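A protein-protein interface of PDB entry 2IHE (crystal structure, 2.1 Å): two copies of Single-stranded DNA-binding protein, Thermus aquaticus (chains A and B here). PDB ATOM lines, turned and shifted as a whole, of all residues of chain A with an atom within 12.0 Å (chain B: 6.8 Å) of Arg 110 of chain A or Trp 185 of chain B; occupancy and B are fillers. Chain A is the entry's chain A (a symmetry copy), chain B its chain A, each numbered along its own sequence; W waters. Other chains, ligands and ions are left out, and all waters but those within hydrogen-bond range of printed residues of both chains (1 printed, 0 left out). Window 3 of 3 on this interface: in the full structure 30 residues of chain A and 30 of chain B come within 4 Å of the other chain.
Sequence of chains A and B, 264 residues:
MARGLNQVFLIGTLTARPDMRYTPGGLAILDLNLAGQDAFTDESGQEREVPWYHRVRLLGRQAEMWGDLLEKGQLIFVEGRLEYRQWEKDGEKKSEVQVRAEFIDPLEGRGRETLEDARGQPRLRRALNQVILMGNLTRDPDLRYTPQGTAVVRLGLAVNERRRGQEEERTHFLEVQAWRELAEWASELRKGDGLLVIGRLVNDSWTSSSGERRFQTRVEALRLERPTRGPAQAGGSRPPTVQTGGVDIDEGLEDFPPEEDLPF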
ATOM      1  N   ILE A  11     -18.575 -19.443  -9.491  1.00  0.00           N
ATOM      2  CA  ILE A  11     -17.519 -20.451  -9.526  1.00  0.00           C
ATOM      3  C   ILE A  11     -16.371 -19.747  -8.814  1.00  0.00           C
ATOM      4  O   ILE A  11     -15.837 -18.749  -9.307  1.00  0.00           O
ATOM      5  CB  ILE A  11     -17.069 -20.848 -10.950  1.00  0.00           C
ATOM      6  CG1 ILE A  11     -18.169 -21.631 -11.663  1.00  0.00           C
ATOM      7  CG2 ILE A  11     -15.857 -21.755 -10.871  1.00  0.00           C
ATOM      8  CD1 ILE A  11     -17.813 -22.048 -13.069  1.00  0.00           C
ATOM      9  N   GLY A  12     -16.040 -20.245  -7.626  1.00  0.00           N
ATOM     10  CA  GLY A  12     -14.973 -19.673  -6.826  1.00  0.00           C
ATOM     11  C   GLY A  12     -14.305 -20.764  -6.023  1.00  0.00           C
ATOM     12  O   GLY A  12     -14.709 -21.928  -6.108  1.00  0.00           O
ATOM     13  N   THR A  13     -13.292 -20.390  -5.244  1.00  0.00           N
ATOM     14  CA  THR A  13     -12.532 -21.346  -4.433  1.00  0.00           C
ATOM     15  C   THR A  13     -12.837 -21.168  -2.951  1.00  0.00           C
ATOM     16  O   THR A  13     -12.939 -20.036  -2.469  1.00  0.00           O
ATOM     17  CB  THR A  13     -10.990 -21.185  -4.646  1.00  0.00           C
ATOM     18  OG1 THR A  13     -10.527 -19.991  -4.004  1.00  0.00           O
ATOM     19  CG2 THR A  13     -10.667 -21.069  -6.125  1.00  0.00           C
ATOM     20  N   GLY A  73      -9.812 -24.493  -0.340  1.00  0.00           N
ATOM     21  CA  GLY A  73      -9.069 -24.507  -1.591  1.00  0.00           C
ATOM     22  C   GLY A  73      -9.803 -25.182  -2.742  1.00  0.00           C
ATOM     23  O   GLY A  73      -9.365 -25.115  -3.892  1.00  0.00           O
ATOM     24  N   GLN A  74     -10.919 -25.838  -2.432  1.00  0.00           N
ATOM     25  CA  GLN A  74     -11.712 -26.503  -3.453  1.00  0.00           C
ATOM     26  C   GLN A  74     -12.484 -25.505  -4.310  1.00  0.00           C
ATOM     27  O   GLN A  74     -13.051 -24.529  -3.811  1.00  0.00           O
ATOM     28  CB  GLN A  74     -12.703 -27.480  -2.821  1.00  0.00           C
ATOM     29  CG  GLN A  74     -12.049 -28.588  -2.035  1.00  0.00           C
ATOM     30  CD  GLN A  74     -12.866 -29.863  -2.039  1.00  0.00           C
ATOM     31  OE1 GLN A  74     -12.623 -30.770  -1.235  1.00  0.00           O
ATOM     32  NE2 GLN A  74     -13.833 -29.949  -2.956  1.00  0.00           N
ATOM     33  N   LEU A  75     -12.493 -25.775  -5.611  1.00  0.00           N
ATOM     34  CA  LEU A  75     -13.194 -24.958  -6.588  1.00  0.00           C
ATOM     35  C   LEU A  75     -14.632 -25.450  -6.573  1.00  0.00           C
ATOM     36  O   LEU A  75     -14.871 -26.651  -6.711  1.00  0.00           O
ATOM     37  CB  LEU A  75     -12.589 -25.188  -7.964  1.00  0.00           C
ATOM     38  CG  LEU A  75     -12.981 -24.207  -9.050  1.00  0.00           C
ATOM     39  CD1 LEU A  75     -12.453 -22.836  -8.659  1.00  0.00           C
ATOM     40  CD2 LEU A  75     -12.413 -24.662 -10.380  1.00  0.00           C
ATOM     41  N   ILE A  76     -15.586 -24.536  -6.419  1.00  0.00           N
ATOM     42  CA  ILE A  76     -16.991 -24.927  -6.357  1.00  0.00           C
ATOM     43  C   ILE A  76     -17.899 -24.167  -7.327  1.00  0.00           C
ATOM     44  O   ILE A  76     -17.713 -22.975  -7.537  1.00  0.00           O
ATOM     45  CB  ILE A  76     -17.552 -24.686  -4.946  1.00  0.00           C
ATOM     46  CG1 ILE A  76     -16.630 -25.301  -3.877  1.00  0.00           C
ATOM     47  CG2 ILE A  76     -18.965 -25.233  -4.866  1.00  0.00           C
ATOM     48  CD1 ILE A  76     -16.648 -26.819  -3.788  1.00  0.00           C
ATOM     49  N   ASP A 105     -21.664 -27.859  -6.815  1.00  0.00           N
ATOM     50  CA  ASP A 105     -20.928 -28.936  -7.453  1.00  0.00           C
ATOM     51  C   ASP A 105     -19.440 -28.680  -7.382  1.00  0.00           C
ATOM     52  O   ASP A 105     -18.919 -27.794  -8.052  1.00  0.00           O
ATOM     53  CB  ASP A 105     -21.352 -29.079  -8.911  1.00  0.00           C
ATOM     54  CG  ASP A 105     -22.745 -29.627  -9.047  1.00  0.00           C
ATOM     55  OD1 ASP A 105     -22.923 -30.850  -8.857  1.00  0.00           O
ATOM     56  OD2 ASP A 105     -23.665 -28.834  -9.325  1.00  0.00           O
ATOM     57  N   PRO A 106     -18.735 -29.428  -6.529  1.00  0.00           N
ATOM     58  CA  PRO A 106     -17.290 -29.214  -6.445  1.00  0.00           C
ATOM     59  C   PRO A 106     -16.710 -29.548  -7.829  1.00  0.00           C
ATOM     60  O   PRO A 106     -17.159 -30.499  -8.472  1.00  0.00           O
ATOM     61  CB  PRO A 106     -16.871 -30.211  -5.365  1.00  0.00           C
ATOM     62  CG  PRO A 106     -18.078 -30.244  -4.464  1.00  0.00           C
ATOM     63  CD  PRO A 106     -19.210 -30.316  -5.452  1.00  0.00           C
ATOM     64  N   LEU A 107     -15.738 -28.772  -8.303  1.00  0.00           N
ATOM     65  CA  LEU A 107     -15.144 -29.029  -9.621  1.00  0.00           C
ATOM     66  C   LEU A 107     -13.689 -29.489  -9.517  1.00  0.00           C
ATOM     67  O   LEU A 107     -12.994 -29.182  -8.541  1.00  0.00           O
ATOM     68  CB  LEU A 107     -15.194 -27.766 -10.494  1.00  0.00           C
ATOM     69  CG  LEU A 107     -16.512 -27.012 -10.684  1.00  0.00           C
ATOM     70  CD1 LEU A 107     -16.207 -25.681 -11.357  1.00  0.00           C
ATOM     71  CD2 LEU A 107     -17.516 -27.847 -11.501  1.00  0.00           C
ATOM     72  N   GLU A 108     -13.224 -30.225 -10.521  1.00  0.00           N
ATOM     73  CA  GLU A 108     -11.841 -30.677 -10.507  1.00  0.00           C
ATOM     74  C   GLU A 108     -10.964 -29.486 -10.870  1.00  0.00           C
ATOM     75  O   GLU A 108     -11.274 -28.736 -11.794  1.00  0.00           O
ATOM     76  CB  GLU A 108     -11.628 -31.812 -11.511  1.00  0.00           C
ATOM     77  CG  GLU A 108     -10.159 -32.238 -11.671  1.00  0.00           C
ATOM     78  CD  GLU A 108      -9.534 -32.819 -10.389  1.00  0.00           C
ATOM     79  OE1 GLU A 108      -9.714 -32.227  -9.297  1.00  0.00           O
ATOM     80  OE2 GLU A 108      -8.843 -33.859 -10.479  1.00  0.00           O
ATOM     81  N   GLY A 109      -9.878 -29.301 -10.130  1.00  0.00           N
ATOM     82  CA  GLY A 109      -8.982 -28.195 -10.410  1.00  0.00           C
ATOM     83  C   GLY A 109      -7.906 -28.560 -11.415  1.00  0.00           C
ATOM     84  O   GLY A 109      -6.997 -27.768 -11.675  1.00  0.00           O
ATOM     85  N   ARG A 110      -8.025 -29.756 -11.987  1.00  0.00           N
ATOM     86  CA  ARG A 110      -7.068 -30.290 -12.964  1.00  0.00           C
ATOM     87  C   ARG A 110      -5.914 -30.259 -11.958  1.00  0.00           C
ATOM     88  O   ARG A 110      -6.026 -30.799 -10.854  1.00  0.00           O
ATOM     89  CB  ARG A 110      -6.859 -29.315 -14.132  1.00  0.00           C
ATOM     90  CG  ARG A 110      -5.888 -29.852 -15.179  1.00  0.00           C
ATOM     91  CD  ARG A 110      -5.611 -28.871 -16.311  1.00  0.00           C
ATOM     92  NE  ARG A 110      -4.726 -29.471 -17.310  1.00  0.00           N
ATOM     93  CZ  ARG A 110      -4.302 -28.858 -18.412  1.00  0.00           C
ATOM     94  NH1 ARG A 110      -4.680 -27.613 -18.668  1.00  0.00           N
ATOM     95  NH2 ARG A 110      -3.497 -29.493 -19.258  1.00  0.00           N
ATOM     96  N   GLY A 111      -4.814 -29.619 -12.349  1.00  0.00           N
ATOM     97  CA  GLY A 111      -3.496 -29.779 -11.752  1.00  0.00           C
ATOM     98  C   GLY A 111      -3.020 -28.523 -11.034  1.00  0.00           C
ATOM     99  O   GLY A 111      -2.800 -28.583  -9.803  1.00  0.00           O
ATOM    100  N   LEU B 143     -11.008 -35.004 -30.985  1.00  0.00           N
ATOM    101  CA  LEU B 143     -10.149 -33.839 -31.183  1.00  0.00           C
ATOM    102  C   LEU B 143      -9.651 -33.817 -32.613  1.00  0.00           C
ATOM    103  O   LEU B 143      -9.213 -34.837 -33.136  1.00  0.00           O
ATOM    104  CB  LEU B 143      -8.946 -33.880 -30.232  1.00  0.00           C
ATOM    105  CG  LEU B 143      -7.942 -32.718 -30.304  1.00  0.00           C
ATOM    106  CD1 LEU B 143      -8.592 -31.450 -29.782  1.00  0.00           C
ATOM    107  CD2 LEU B 143      -6.702 -33.035 -29.476  1.00  0.00           C
ATOM    108  N   LEU B 155     -18.145 -32.762 -28.865  1.00  0.00           N
ATOM    109  CA  LEU B 155     -18.551 -33.583 -27.730  1.00  0.00           C
ATOM    110  C   LEU B 155     -20.037 -33.893 -27.767  1.00  0.00           C
ATOM    111  O   LEU B 155     -20.833 -33.050 -28.166  1.00  0.00           O
ATOM    112  CB  LEU B 155     -18.246 -32.843 -26.422  1.00  0.00           C
ATOM    113  CG  LEU B 155     -16.819 -32.352 -26.180  1.00  0.00           C
ATOM    114  CD1 LEU B 155     -16.825 -31.303 -25.093  1.00  0.00           C
ATOM    115  CD2 LEU B 155     -15.931 -33.531 -25.808  1.00  0.00           C
ATOM    116  N   ARG B 180      -9.210 -24.408 -29.521  1.00  0.00           N
ATOM    117  CA  ARG B 180      -7.899 -24.146 -28.949  1.00  0.00           C
ATOM    118  C   ARG B 180      -7.642 -24.819 -27.606  1.00  0.00           C
ATOM    119  O   ARG B 180      -7.794 -26.034 -27.456  1.00  0.00           O
ATOM    120  CB  ARG B 180      -7.723 -22.635 -28.799  1.00  0.00           C
ATOM    121  CG  ARG B 180      -8.219 -21.840 -30.011  1.00  0.00           C
ATOM    122  CD  ARG B 180      -8.133 -20.326 -29.792  1.00  0.00           C
ATOM    123  NE  ARG B 180      -8.458 -19.571 -31.003  1.00  0.00           N
ATOM    124  CZ  ARG B 180      -9.677 -19.469 -31.531  1.00  0.00           C
ATOM    125  NH1 ARG B 180     -10.712 -20.070 -30.958  1.00  0.00           N
ATOM    126  NH2 ARG B 180      -9.862 -18.764 -32.641  1.00  0.00           N
ATOM    127  N   GLU B 181      -7.236 -24.005 -26.639  1.00  0.00           N
ATOM    128  CA  GLU B 181      -6.936 -24.469 -25.295  1.00  0.00           C
ATOM    129  C   GLU B 181      -8.031 -25.355 -24.711  1.00  0.00           C
ATOM    130  O   GLU B 181      -7.731 -26.417 -24.178  1.00  0.00           O
ATOM    131  CB  GLU B 181      -6.704 -23.268 -24.392  1.00  0.00           C
ATOM    132  CG  GLU B 181      -7.877 -22.307 -24.361  1.00  0.00           C
ATOM    133  CD  GLU B 181      -7.453 -20.864 -24.542  1.00  0.00           C
ATOM    134  OE1 GLU B 181      -8.310 -19.971 -24.370  1.00  0.00           O
ATOM    135  OE2 GLU B 181      -6.265 -20.627 -24.861  1.00  0.00           O
ATOM    136  N   LEU B 182      -9.291 -24.922 -24.805  1.00  0.00           N
ATOM    137  CA  LEU B 182     -10.415 -25.710 -24.277  1.00  0.00           C
ATOM    138  C   LEU B 182     -10.552 -27.061 -24.953  1.00  0.00           C
ATOM    139  O   LEU B 182     -10.823 -28.063 -24.293  1.00  0.00           O
ATOM    140  CB  LEU B 182     -11.749 -24.966 -24.419  1.00  0.00           C
ATOM    141  CG  LEU B 182     -12.197 -24.034 -23.298  1.00  0.00           C
ATOM    142  CD1 LEU B 182     -13.623 -23.587 -23.555  1.00  0.00           C
ATOM    143  CD2 LEU B 182     -12.110 -24.760 -21.966  1.00  0.00           C
ATOM    144  N   ALA B 183     -10.368 -27.084 -26.271  1.00  0.00           N
ATOM    145  CA  ALA B 183     -10.474 -28.322 -27.036  1.00  0.00           C
ATOM    146  C   ALA B 183      -9.435 -29.335 -26.570  1.00  0.00           C
ATOM    147  O   ALA B 183      -9.753 -30.500 -26.342  1.00  0.00           O
ATOM    148  CB  ALA B 183     -10.296 -28.032 -28.528  1.00  0.00           C
ATOM    149  N   GLU B 184      -8.192 -28.891 -26.425  1.00  0.00           N
ATOM    150  CA  GLU B 184      -7.139 -29.799 -25.999  1.00  0.00           C
ATOM    151  C   GLU B 184      -7.356 -30.332 -24.585  1.00  0.00           C
ATOM    152  O   GLU B 184      -6.981 -31.466 -24.284  1.00  0.00           O
ATOM    153  CB  GLU B 184      -5.775 -29.123 -26.119  1.00  0.00           C
ATOM    154  CG  GLU B 184      -5.425 -28.763 -27.545  1.00  0.00           C
ATOM    155  CD  GLU B 184      -3.938 -28.570 -27.743  1.00  0.00           C
ATOM    156  OE1 GLU B 184      -3.323 -27.859 -26.924  1.00  0.00           O
ATOM    157  OE2 GLU B 184      -3.388 -29.127 -28.716  1.00  0.00           O
ATOM    158  N   TRP B 185      -7.954 -29.512 -23.719  1.00  0.00           N
ATOM    159  CA  TRP B 185      -8.251 -29.923 -22.343  1.00  0.00           C
ATOM    160  C   TRP B 185      -9.368 -30.964 -22.401  1.00  0.00           C
ATOM    161  O   TRP B 185      -9.286 -31.999 -21.739  1.00  0.00           O
ATOM    162  CB  TRP B 185      -8.719 -28.723 -21.505  1.00  0.00           C
ATOM    163  CG  TRP B 185      -9.250 -29.064 -20.109  1.00  0.00           C
ATOM    164  CD1 TRP B 185      -8.535 -29.115 -18.939  1.00  0.00           C
ATOM    165  CD2 TRP B 185     -10.610 -29.392 -19.758  1.00  0.00           C
ATOM    166  NE1 TRP B 185      -9.363 -29.448 -17.886  1.00  0.00           N
ATOM    167  CE2 TRP B 185     -10.637 -29.623 -18.358  1.00  0.00           C
ATOM    168  CE3 TRP B 185     -11.806 -29.510 -20.490  1.00  0.00           C
ATOM    169  CZ2 TRP B 185     -11.815 -29.971 -17.677  1.00  0.00           C
ATOM    170  CZ3 TRP B 185     -12.976 -29.858 -19.812  1.00  0.00           C
ATOM    171  CH2 TRP B 185     -12.970 -30.082 -18.417  1.00  0.00           C
ATOM    172  N   ALA B 186     -10.401 -30.686 -23.201  1.00  0.00           N
ATOM    173  CA  ALA B 186     -11.553 -31.585 -23.348  1.00  0.00           C
ATOM    174  C   ALA B 186     -11.206 -32.922 -23.989  1.00  0.00           C
ATOM    175  O   ALA B 186     -11.932 -33.899 -23.817  1.00  0.00           O
ATOM    176  CB  ALA B 186     -12.657 -30.902 -24.157  1.00  0.00           C
ATOM    177  N   SER B 187     -10.106 -32.968 -24.732  1.00  0.00           N
ATOM    178  CA  SER B 187      -9.697 -34.205 -25.384  1.00  0.00           C
ATOM    179  C   SER B 187      -9.270 -35.260 -24.356  1.00  0.00           C
ATOM    180  O   SER B 187      -9.162 -36.445 -24.686  1.00  0.00           O
ATOM    181  CB  SER B 187      -8.547 -33.937 -26.365  1.00  0.00           C
ATOM    182  OG  SER B 187      -7.390 -33.459 -25.694  1.00  0.00           O
ATOM    183  N   GLU B 188      -9.048 -34.823 -23.112  1.00  0.00           N
ATOM    184  CA  GLU B 188      -8.624 -35.704 -22.013  1.00  0.00           C
ATOM    185  C   GLU B 188      -9.817 -36.299 -21.229  1.00  0.00           C
ATOM    186  O   GLU B 188      -9.638 -37.072 -20.283  1.00  0.00           O
ATOM    187  CB  GLU B 188      -7.698 -34.920 -21.064  1.00  0.00           C
ATOM    188  CG  GLU B 188      -6.837 -35.770 -20.130  1.00  0.00           C
ATOM    189  CD  GLU B 188      -5.947 -34.932 -19.205  1.00  0.00           C
ATOM    190  OE1 GLU B 188      -5.156 -34.105 -19.711  1.00  0.00           O
ATOM    191  OE2 GLU B 188      -6.038 -35.108 -17.969  1.00  0.00           O
ATOM    192  N   LEU B 189     -11.031 -35.932 -21.629  1.00  0.00           N
ATOM    193  CA  LEU B 189     -12.245 -36.424 -20.986  1.00  0.00           C
ATOM    194  C   LEU B 189     -12.577 -37.830 -21.489  1.00  0.00           C
ATOM    195  O   LEU B 189     -12.079 -38.256 -22.535  1.00  0.00           O
ATOM    196  CB  LEU B 189     -13.421 -35.501 -21.303  1.00  0.00           C
ATOM    197  CG  LEU B 189     -13.520 -34.144 -20.633  1.00  0.00           C
ATOM    198  CD1 LEU B 189     -14.562 -33.323 -21.378  1.00  0.00           C
ATOM    199  CD2 LEU B 189     -13.879 -34.311 -19.161  1.00  0.00           C
ATOM    200  N   GLY B 194     -18.773 -36.329 -16.211  1.00  0.00           N
ATOM    201  CA  GLY B 194     -19.716 -35.246 -16.011  1.00  0.00           C
ATOM    202  C   GLY B 194     -19.090 -34.001 -16.604  1.00  0.00           C
ATOM    203  O   GLY B 194     -17.867 -33.839 -16.557  1.00  0.00           O
ATOM    204  N   LEU B 195     -19.904 -33.116 -17.167  1.00  0.00           N
ATOM    205  CA  LEU B 195     -19.355 -31.913 -17.764  1.00  0.00           C
ATOM    206  C   LEU B 195     -20.257 -30.706 -17.561  1.00  0.00           C
ATOM    207  O   LEU B 195     -21.469 -30.805 -17.733  1.00  0.00           O
ATOM    208  CB  LEU B 195     -19.121 -32.146 -19.265  1.00  0.00           C
ATOM    209  CG  LEU B 195     -18.468 -31.033 -20.102  1.00  0.00           C
ATOM    210  CD1 LEU B 195     -17.080 -30.729 -19.550  1.00  0.00           C
ATOM    211  CD2 LEU B 195     -18.375 -31.462 -21.567  1.00  0.00           C
ATOM    212  N   LEU B 196     -19.659 -29.577 -17.175  1.00  0.00           N
ATOM    213  CA  LEU B 196     -20.393 -28.325 -17.007  1.00  0.00           C
ATOM    214  C   LEU B 196     -20.029 -27.483 -18.220  1.00  0.00           C
ATOM    215  O   LEU B 196     -18.848 -27.256 -18.486  1.00  0.00           O
ATOM    216  CB  LEU B 196     -19.975 -27.582 -15.729  1.00  0.00           C
ATOM    217  CG  LEU B 196     -20.564 -26.173 -15.519  1.00  0.00           C
ATOM    218  CD1 LEU B 196     -22.080 -26.244 -15.365  1.00  0.00           C
ATOM    219  CD2 LEU B 196     -19.932 -25.545 -14.286  1.00  0.00           C
ATOM    220  N   LEU B 224     -15.601 -24.557 -19.916  1.00  0.00           N
ATOM    221  CA  LEU B 224     -15.831 -25.966 -19.573  1.00  0.00           C
ATOM    222  C   LEU B 224     -15.185 -26.359 -18.237  1.00  0.00           C
ATOM    223  O   LEU B 224     -14.066 -25.940 -17.927  1.00  0.00           O
ATOM    224  CB  LEU B 224     -15.313 -26.896 -20.685  1.00  0.00           C
ATOM    225  CG  LEU B 224     -15.944 -26.889 -22.086  1.00  0.00           C
ATOM    226  CD1 LEU B 224     -15.255 -27.938 -22.944  1.00  0.00           C
ATOM    227  CD2 LEU B 224     -17.421 -27.181 -22.004  1.00  0.00           C
ATOM    228  N   GLU B 225     -15.899 -27.163 -17.451  1.00  0.00           N
ATOM    229  CA  GLU B 225     -15.402 -27.622 -16.151  1.00  0.00           C
ATOM    230  C   GLU B 225     -15.903 -29.037 -15.903  1.00  0.00           C
ATOM    231  O   GLU B 225     -16.965 -29.417 -16.382  1.00  0.00           O
ATOM    232  CB  GLU B 225     -15.910 -26.728 -15.022  1.00  0.00           C
ATOM    233  CG  GLU B 225     -15.546 -25.242 -15.134  1.00  0.00           C
ATOM    234  CD  GLU B 225     -14.054 -24.963 -15.001  1.00  0.00           C
ATOM    235  OE1 GLU B 225     -13.317 -25.829 -14.484  1.00  0.00           O
ATOM    236  OE2 GLU B 225     -13.625 -23.864 -15.403  1.00  0.00           O
ATOM    237  N   ARG B 226     -15.130 -29.817 -15.163  1.00  0.00           N
ATOM    238  CA  ARG B 226     -15.517 -31.175 -14.856  1.00  0.00           C
ATOM    239  C   ARG B 226     -15.936 -31.276 -13.392  1.00  0.00           C
ATOM    240  O   ARG B 226     -15.131 -31.049 -12.474  1.00  0.00           O
ATOM    241  CB  ARG B 226     -14.364 -32.141 -15.149  1.00  0.00           C
ATOM    242  CG  ARG B 226     -14.815 -33.353 -15.941  1.00  0.00           C
ATOM    243  CD  ARG B 226     -14.686 -34.619 -15.131  1.00  0.00           C
ATOM    244  NE  ARG B 226     -13.291 -34.861 -14.788  1.00  0.00           N
ATOM    245  CZ  ARG B 226     -12.886 -35.756 -13.898  1.00  0.00           C
ATOM    246  NH1 ARG B 226     -13.772 -36.505 -13.255  1.00  0.00           N
ATOM    247  NH2 ARG B 226     -11.593 -35.888 -13.634  1.00  0.00           N
HETATM  248  O   HOH W   1     -12.794 -28.563 -14.288  1.00  0.00           O
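O of Arg 226 of chain B lies within hydrogen-bond range of N of Glu 108 of chain A.
Leu 75 of chain A touches none of the printed residues of chain B.
Of the printed residues of chain B, Leu 107 of chain A touches Glu 225 (3.8 Å) and Arg 226 (3.5 Å).
Printed residues of chain B within 4 Å of Glu 108 of chain A: Arg 226 (2.9 Å).
No residue of chain B comes within 4 Å of Gly 109 of chain A.
Arg 110 of chain A touches one residue of chain B.
Ala 183 of chain B touches none of the printed residues of chain A.
No residue of chain A comes within 4 Å of Glu 184 of chain B.
Trp 185 of chain B touches just one residue of chain A: Arg 110.
No residue of chain A comes within 4 Å of Ser 187 of chain B.
No residue of chain A comes within 4 Å of Glu 188 of chain B.
No residue of chain A comes within 4 Å of Leu 189 of chain B.
No residue of chain A comes within 4 Å of Leu 224 of chain B.
Of chain A, only Leu 107 (3.8 Å) comes within 4 Å of Glu 225 of chain B.
Printed residues of chain A within 4 Å of Arg 226 of chain B: Leu 107 and Glu 108.
Water W1 lies within hydrogen-bond range of OE1 of Glu 225 of chain B (2.8 Å), N of Arg 226 of chain B (2.8 Å) and O of Glu 108 of chain A (2.9 Å).
Among the printed residues, pairs that only touch across the chains: Leu 107 of chain A with Glu 225 of chain B (3.8 Å), Leu 107 of chain A with Arg 226 of chain B (3.5 Å) and Arg 110 of chain A with Trp 185 of chain B (3.9 Å).
No position is printed for both chains.
The backbone carbonyl oxygen of Glu 225 of chain B lies within hydrogen-bond range of the backbone NH of Leu 196 of chain B (2.8 Å).
The backbone carbonyl oxygen (O) of Leu 75 of chain A is in hydrogen-bond range of the backbone NH (N) of Leu 107 of chain A (2.8 Å).
Of the 18 printed residues of chain B, 3 touch a printed residue of chain A.
Printed residues of chain B that touch a printed residue of chain A: Trp 185, Glu 225 and Arg 226.
Hydrophobic or aromatic side chains of chain B within 4 Å of the printed part of chain A: Trp 185.
Among the printed residues, 4 pairs touch across the chains.
Among the printed residues, no Asp or Glu carboxylate lies within 4 Å of a Lys or Arg side-chain nitrogen of the other chain.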
